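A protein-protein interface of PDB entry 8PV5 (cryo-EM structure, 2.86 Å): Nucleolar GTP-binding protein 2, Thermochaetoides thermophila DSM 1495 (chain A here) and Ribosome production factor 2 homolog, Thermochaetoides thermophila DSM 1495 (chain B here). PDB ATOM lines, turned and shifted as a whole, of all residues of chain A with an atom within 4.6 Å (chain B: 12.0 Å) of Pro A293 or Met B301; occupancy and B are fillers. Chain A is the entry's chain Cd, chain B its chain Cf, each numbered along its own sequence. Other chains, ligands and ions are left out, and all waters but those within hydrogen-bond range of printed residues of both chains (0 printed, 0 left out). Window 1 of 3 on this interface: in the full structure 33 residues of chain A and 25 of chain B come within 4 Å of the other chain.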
ATOM      1  N   PRO A 102     -12.225 -25.062  21.438  1.00  0.00           N
ATOM      2  CA  PRO A 102     -10.964 -24.300  21.365  1.00  0.00           C
ATOM      3  C   PRO A 102      -9.784 -24.960  22.059  1.00  0.00           C
ATOM      4  O   PRO A 102      -8.640 -24.722  21.653  1.00  0.00           O
ATOM      5  CB  PRO A 102     -11.321 -22.967  22.038  1.00  0.00           C
ATOM      6  CG  PRO A 102     -12.805 -22.872  21.937  1.00  0.00           C
ATOM      7  CD  PRO A 102     -13.304 -24.277  22.059  1.00  0.00           C
ATOM      8  N   TYR A 103     -10.013 -25.777  23.084  1.00  0.00           N
ATOM      9  CA  TYR A 103      -8.932 -26.358  23.867  1.00  0.00           C
ATOM     10  C   TYR A 103      -8.439 -27.686  23.311  1.00  0.00           C
ATOM     11  O   TYR A 103      -7.670 -28.379  23.983  1.00  0.00           O
ATOM     12  CB  TYR A 103      -9.370 -26.530  25.322  1.00  0.00           C
ATOM     13  CG  TYR A 103      -9.980 -25.282  25.913  1.00  0.00           C
ATOM     14  CD1 TYR A 103      -9.259 -24.096  25.973  1.00  0.00           C
ATOM     15  CD2 TYR A 103     -11.279 -25.286  26.405  1.00  0.00           C
ATOM     16  CE1 TYR A 103      -9.812 -22.951  26.509  1.00  0.00           C
ATOM     17  CE2 TYR A 103     -11.841 -24.145  26.943  1.00  0.00           C
ATOM     18  CZ  TYR A 103     -11.104 -22.981  26.991  1.00  0.00           C
ATOM     19  OH  TYR A 103     -11.661 -21.844  27.527  1.00  0.00           O
ATOM     20  N   LEU A 266      -2.884 -22.149  16.925  1.00  0.00           N
ATOM     21  CA  LEU A 266      -2.970 -20.706  17.109  1.00  0.00           C
ATOM     22  C   LEU A 266      -3.385 -20.403  18.542  1.00  0.00           C
ATOM     23  O   LEU A 266      -4.432 -20.874  19.001  1.00  0.00           O
ATOM     24  CB  LEU A 266      -3.960 -20.093  16.120  1.00  0.00           C
ATOM     25  CG  LEU A 266      -4.243 -18.596  16.255  1.00  0.00           C
ATOM     26  CD1 LEU A 266      -2.962 -17.795  16.147  1.00  0.00           C
ATOM     27  CD2 LEU A 266      -5.237 -18.149  15.202  1.00  0.00           C
ATOM     28  N   VAL A 267      -2.563 -19.628  19.246  1.00  0.00           N
ATOM     29  CA  VAL A 267      -2.823 -19.225  20.623  1.00  0.00           C
ATOM     30  C   VAL A 267      -2.665 -17.713  20.716  1.00  0.00           C
ATOM     31  O   VAL A 267      -1.685 -17.151  20.214  1.00  0.00           O
ATOM     32  CB  VAL A 267      -1.876 -19.944  21.612  1.00  0.00           C
ATOM     33  CG1 VAL A 267      -2.024 -19.389  23.019  1.00  0.00           C
ATOM     34  CG2 VAL A 267      -2.129 -21.444  21.611  1.00  0.00           C
ATOM     35  N   PHE A 268      -3.640 -17.052  21.337  1.00  0.00           N
ATOM     36  CA  PHE A 268      -3.568 -15.616  21.563  1.00  0.00           C
ATOM     37  C   PHE A 268      -2.776 -15.325  22.830  1.00  0.00           C
ATOM     38  O   PHE A 268      -2.863 -16.061  23.814  1.00  0.00           O
ATOM     39  CB  PHE A 268      -4.968 -15.010  21.685  1.00  0.00           C
ATOM     40  CG  PHE A 268      -5.773 -15.075  20.422  1.00  0.00           C
ATOM     41  CD1 PHE A 268      -5.182 -14.833  19.194  1.00  0.00           C
ATOM     42  CD2 PHE A 268      -7.126 -15.357  20.467  1.00  0.00           C
ATOM     43  CE1 PHE A 268      -5.925 -14.885  18.032  1.00  0.00           C
ATOM     44  CE2 PHE A 268      -7.875 -15.411  19.309  1.00  0.00           C
ATOM     45  CZ  PHE A 268      -7.273 -15.175  18.090  1.00  0.00           C
ATOM     46  N   HIS A 292      -9.983 -18.932  20.501  1.00  0.00           N
ATOM     47  CA  HIS A 292      -8.701 -19.599  20.678  1.00  0.00           C
ATOM     48  C   HIS A 292      -8.263 -19.491  22.130  1.00  0.00           C
ATOM     49  O   HIS A 292      -8.701 -18.580  22.841  1.00  0.00           O
ATOM     50  CB  HIS A 292      -7.626 -18.988  19.764  1.00  0.00           C
ATOM     51  CG  HIS A 292      -7.852 -19.248  18.308  1.00  0.00           C
ATOM     52  ND1 HIS A 292      -8.528 -18.368  17.492  1.00  0.00           N
ATOM     53  CD2 HIS A 292      -7.491 -20.289  17.522  1.00  0.00           C
ATOM     54  CE1 HIS A 292      -8.575 -18.856  16.264  1.00  0.00           C
ATOM     55  NE2 HIS A 292      -7.951 -20.020  16.256  1.00  0.00           N
ATOM     56  N   PRO A 293      -7.428 -20.417  22.606  1.00  0.00           N
ATOM     57  CA  PRO A 293      -6.849 -20.266  23.949  1.00  0.00           C
ATOM     58  C   PRO A 293      -6.006 -19.004  24.055  1.00  0.00           C
ATOM     59  O   PRO A 293      -5.267 -18.649  23.134  1.00  0.00           O
ATOM     60  CB  PRO A 293      -5.998 -21.530  24.108  1.00  0.00           C
ATOM     61  CG  PRO A 293      -6.602 -22.514  23.187  1.00  0.00           C
ATOM     62  CD  PRO A 293      -7.119 -21.733  22.021  1.00  0.00           C
ATOM     63  N   THR A 294      -6.116 -18.329  25.198  1.00  0.00           N
ATOM     64  CA  THR A 294      -5.539 -17.009  25.393  1.00  0.00           C
ATOM     65  C   THR A 294      -4.737 -16.971  26.686  1.00  0.00           C
ATOM     66  O   THR A 294      -5.218 -17.404  27.737  1.00  0.00           O
ATOM     67  CB  THR A 294      -6.635 -15.936  25.433  1.00  0.00           C
ATOM     68  OG1 THR A 294      -7.494 -16.094  24.300  1.00  0.00           O
ATOM     69  CG2 THR A 294      -6.031 -14.545  25.398  1.00  0.00           C
ATOM     70  N   CYS A 295      -3.522 -16.438  26.603  1.00  0.00           N
ATOM     71  CA  CYS A 295      -2.658 -16.241  27.757  1.00  0.00           C
ATOM     72  C   CYS A 295      -2.494 -14.752  28.023  1.00  0.00           C
ATOM     73  O   CYS A 295      -2.062 -14.005  27.144  1.00  0.00           O
ATOM     74  CB  CYS A 295      -1.276 -16.867  27.538  1.00  0.00           C
ATOM     75  SG  CYS A 295      -1.265 -18.644  27.257  1.00  0.00           S
ATOM     76  N   SER A 309       2.409 -19.645  33.181  1.00  0.00           N
ATOM     77  CA  SER A 309       1.309 -20.212  32.407  1.00  0.00           C
ATOM     78  C   SER A 309       1.697 -20.408  30.945  1.00  0.00           C
ATOM     79  O   SER A 309       1.397 -21.451  30.346  1.00  0.00           O
ATOM     80  CB  SER A 309       0.076 -19.317  32.522  1.00  0.00           C
ATOM     81  OG  SER A 309      -0.942 -19.741  31.633  1.00  0.00           O
ATOM     82  N   LEU A 313       2.049 -23.992  28.986  1.00  0.00           N
ATOM     83  CA  LEU A 313       1.347 -24.298  27.741  1.00  0.00           C
ATOM     84  C   LEU A 313       2.318 -24.780  26.663  1.00  0.00           C
ATOM     85  O   LEU A 313       2.023 -25.728  25.919  1.00  0.00           O
ATOM     86  CB  LEU A 313       0.571 -23.069  27.269  1.00  0.00           C
ATOM     87  CG  LEU A 313      -0.222 -23.225  25.974  1.00  0.00           C
ATOM     88  CD1 LEU A 313      -1.195 -24.381  26.088  1.00  0.00           C
ATOM     89  CD2 LEU A 313      -0.957 -21.947  25.630  1.00  0.00           C
ATOM     90  N   ASN B 286      -3.732 -37.261  27.231  1.00  0.00           N
ATOM     91  CA  ASN B 286      -4.140 -36.119  26.416  1.00  0.00           C
ATOM     92  C   ASN B 286      -4.059 -36.386  24.917  1.00  0.00           C
ATOM     93  O   ASN B 286      -3.962 -35.439  24.131  1.00  0.00           O
ATOM     94  CB  ASN B 286      -3.338 -34.858  26.761  1.00  0.00           C
ATOM     95  CG  ASN B 286      -3.417 -34.505  28.229  1.00  0.00           C
ATOM     96  OD1 ASN B 286      -4.461 -34.079  28.721  1.00  0.00           O
ATOM     97  ND2 ASN B 286      -2.309 -34.676  28.938  1.00  0.00           N
ATOM     98  N   ILE B 296      -6.212 -36.112  18.103  1.00  0.00           N
ATOM     99  CA  ILE B 296      -6.552 -34.882  18.801  1.00  0.00           C
ATOM    100  C   ILE B 296      -5.751 -34.810  20.093  1.00  0.00           C
ATOM    101  O   ILE B 296      -5.693 -35.783  20.854  1.00  0.00           O
ATOM    102  CB  ILE B 296      -8.067 -34.804  19.090  1.00  0.00           C
ATOM    103  CG1 ILE B 296      -8.866 -34.981  17.800  1.00  0.00           C
ATOM    104  CG2 ILE B 296      -8.426 -33.491  19.748  1.00  0.00           C
ATOM    105  CD1 ILE B 296      -8.563 -33.936  16.752  1.00  0.00           C
ATOM    106  N   GLY B 297      -5.128 -33.661  20.330  1.00  0.00           N
ATOM    107  CA  GLY B 297      -4.420 -33.392  21.566  1.00  0.00           C
ATOM    108  C   GLY B 297      -5.221 -32.451  22.443  1.00  0.00           C
ATOM    109  O   GLY B 297      -5.967 -31.605  21.948  1.00  0.00           O
ATOM    110  N   ARG B 298      -5.067 -32.606  23.754  1.00  0.00           N
ATOM    111  CA  ARG B 298      -5.767 -31.787  24.733  1.00  0.00           C
ATOM    112  C   ARG B 298      -4.769 -30.896  25.455  1.00  0.00           C
ATOM    113  O   ARG B 298      -3.792 -31.390  26.026  1.00  0.00           O
ATOM    114  CB  ARG B 298      -6.512 -32.659  25.746  1.00  0.00           C
ATOM    115  CG  ARG B 298      -7.989 -32.836  25.454  1.00  0.00           C
ATOM    116  CD  ARG B 298      -8.798 -31.636  25.908  1.00  0.00           C
ATOM    117  NE  ARG B 298     -10.226 -31.846  25.699  1.00  0.00           N
ATOM    118  CZ  ARG B 298     -11.156 -30.919  25.880  1.00  0.00           C
ATOM    119  NH1 ARG B 298     -10.846 -29.694  26.269  1.00  0.00           N
ATOM    120  NH2 ARG B 298     -12.431 -31.228  25.659  1.00  0.00           N
ATOM    121  N   ILE B 299      -5.017 -29.590  25.431  1.00  0.00           N
ATOM    122  CA  ILE B 299      -4.210 -28.631  26.173  1.00  0.00           C
ATOM    123  C   ILE B 299      -5.053 -28.093  27.316  1.00  0.00           C
ATOM    124  O   ILE B 299      -6.286 -28.051  27.240  1.00  0.00           O
ATOM    125  CB  ILE B 299      -3.685 -27.482  25.285  1.00  0.00           C
ATOM    126  CG1 ILE B 299      -4.839 -26.785  24.566  1.00  0.00           C
ATOM    127  CG2 ILE B 299      -2.678 -28.009  24.282  1.00  0.00           C
ATOM    128  CD1 ILE B 299      -4.406 -25.615  23.716  1.00  0.00           C
ATOM    129  N   HIS B 300      -4.380 -27.688  28.388  1.00  0.00           N
ATOM    130  CA  HIS B 300      -5.046 -27.264  29.615  1.00  0.00           C
ATOM    131  C   HIS B 300      -4.484 -25.914  30.030  1.00  0.00           C
ATOM    132  O   HIS B 300      -3.275 -25.775  30.241  1.00  0.00           O
ATOM    133  CB  HIS B 300      -4.870 -28.315  30.706  1.00  0.00           C
ATOM    134  CG  HIS B 300      -5.282 -29.687  30.274  1.00  0.00           C
ATOM    135  ND1 HIS B 300      -6.590 -30.117  30.317  1.00  0.00           N
ATOM    136  CD2 HIS B 300      -4.562 -30.717  29.772  1.00  0.00           C
ATOM    137  CE1 HIS B 300      -6.657 -31.355  29.863  1.00  0.00           C
ATOM    138  NE2 HIS B 300      -5.439 -31.746  29.533  1.00  0.00           N
ATOM    139  N   MET B 301      -5.365 -24.920  30.135  1.00  0.00           N
ATOM    140  CA  MET B 301      -4.917 -23.552  30.358  1.00  0.00           C
ATOM    141  C   MET B 301      -4.756 -23.261  31.844  1.00  0.00           C
ATOM    142  O   MET B 301      -3.767 -22.651  32.266  1.00  0.00           O
ATOM    143  CB  MET B 301      -5.906 -22.575  29.724  1.00  0.00           C
ATOM    144  CG  MET B 301      -5.974 -22.663  28.211  1.00  0.00           C
ATOM    145  SD  MET B 301      -4.405 -22.298  27.421  1.00  0.00           S
ATOM    146  CE  MET B 301      -4.292 -20.558  27.777  1.00  0.00           C
ATOM    147  N   GLY B 302      -5.716 -23.691  32.651  1.00  0.00           N
ATOM    148  CA  GLY B 302      -5.739 -23.361  34.058  1.00  0.00           C
ATOM    149  C   GLY B 302      -6.568 -22.118  34.339  1.00  0.00           C
ATOM    150  O   GLY B 302      -6.931 -21.353  33.441  1.00  0.00           O
ATOM    151  N   LYS B 303      -6.877 -21.924  35.617  1.00  0.00           N
ATOM    152  CA  LYS B 303      -7.687 -20.788  36.031  1.00  0.00           C
ATOM    153  C   LYS B 303      -6.898 -19.491  35.908  1.00  0.00           C
ATOM    154  O   LYS B 303      -5.747 -19.400  36.344  1.00  0.00           O
ATOM    155  CB  LYS B 303      -8.165 -20.977  37.470  1.00  0.00           C
ATOM    156  N   THR B 304      -7.526 -18.483  35.308  1.00  0.00           N
ATOM    157  CA  THR B 304      -6.892 -17.183  35.132  1.00  0.00           C
ATOM    158  C   THR B 304      -6.974 -16.401  36.436  1.00  0.00           C
ATOM    159  O   THR B 304      -8.063 -15.998  36.859  1.00  0.00           O
ATOM    160  CB  THR B 304      -7.562 -16.410  33.998  1.00  0.00           C
ATOM    161  N   ASP B 305      -5.824 -16.181  37.070  1.00  0.00           N
ATOM    162  CA  ASP B 305      -5.749 -15.489  38.356  1.00  0.00           C
ATOM    163  C   ASP B 305      -4.970 -14.195  38.155  1.00  0.00           C
ATOM    164  O   ASP B 305      -3.736 -14.191  38.206  1.00  0.00           O
ATOM    165  CB  ASP B 305      -5.098 -16.369  39.418  1.00  0.00           C
ATOM    166  N   LEU B 306      -5.690 -13.100  37.928  1.00  0.00           N
ATOM    167  CA  LEU B 306      -5.091 -11.786  37.754  1.00  0.00           C
ATOM    168  C   LEU B 306      -5.168 -10.938  39.016  1.00  0.00           C
ATOM    169  O   LEU B 306      -4.953  -9.724  38.945  1.00  0.00           O
ATOM    170  CB  LEU B 306      -5.763 -11.042  36.595  1.00  0.00           C
ATOM    171  CG  LEU B 306      -5.182 -11.139  35.179  1.00  0.00           C
ATOM    172  CD1 LEU B 306      -4.982 -12.577  34.727  1.00  0.00           C
ATOM    173  CD2 LEU B 306      -6.073 -10.394  34.200  1.00  0.00           C
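The backbone carbonyl oxygen of Tyr A103 is in hydrogen-bond range of the backbone NH of Ile B299 (3.3 Å).
The backbone carbonyl oxygen (O) of Pro A293 is in hydrogen-bond range of the backbone NH (N) of Phe A268, at 2.9 Å. The backbone NH (N) of Cys A295 is in hydrogen-bond range of the backbone carbonyl oxygen (O) of Phe A268, 2.9 Å away. The backbone carbonyl oxygen of His A292 lies within hydrogen-bond range of the side-chain hydroxyl of Thr A294. The backbone NH of Arg B298 is in hydrogen-bond range of the backbone carbonyl oxygen of Asn B286 (3.1 Å).
CB of Tyr A103 touches NH1 of Arg B298 (3.6 Å). Pro A293 touches Ile B299. Met B301 touches Pro A293. Met B301 touches Thr A294 (CE to O, 3.3 Å). CE of Met B301 touches SG of Cys A295 (3.6 Å). SD of Met B301 touches CD2 of Leu A313, at 3.9 Å.
No residue of chain B comes within 4 Å of Pro A102. No residue of chain B comes within 4 Å of Leu A266. No residue of chain B comes within 4 Å of Val A267. No residue of chain B comes within 4 Å of Phe A268. No residue of chain B comes within 4 Å of His A292. Thr A294 touches just one residue of chain B: Met B301 (3.3 Å). Of chain B, only Met B301 (3.6 Å) comes within 4 Å of Cys A295. Leu A313 touches one residue of chain B. Of the printed residues of chain A, Arg B298 touches Tyr A103. Of the printed residues of chain A, Ile B299 touches Tyr A103 (3.3 Å) and Pro A293 (3.8 Å). Of chain A, only Pro A293, Thr A294, Cys A295 and Leu A313 come within 4 Å of Met B301. Asp B305 touches none of the printed residues of chain A. The nearest printed residue of chain A that does not touch Ile B299 is Leu A313 (4.1 Å).
Printed residues of chain B that touch a printed residue of chain A: Arg B298, Ile B299 and Met B301. Of the 11 printed residues of chain A, 5 touch a printed residue of chain B. Along chain A the printed residues that touch a printed residue of chain B span positions 103 to 313. Among the printed residues, 7 pairs touch across the chains.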
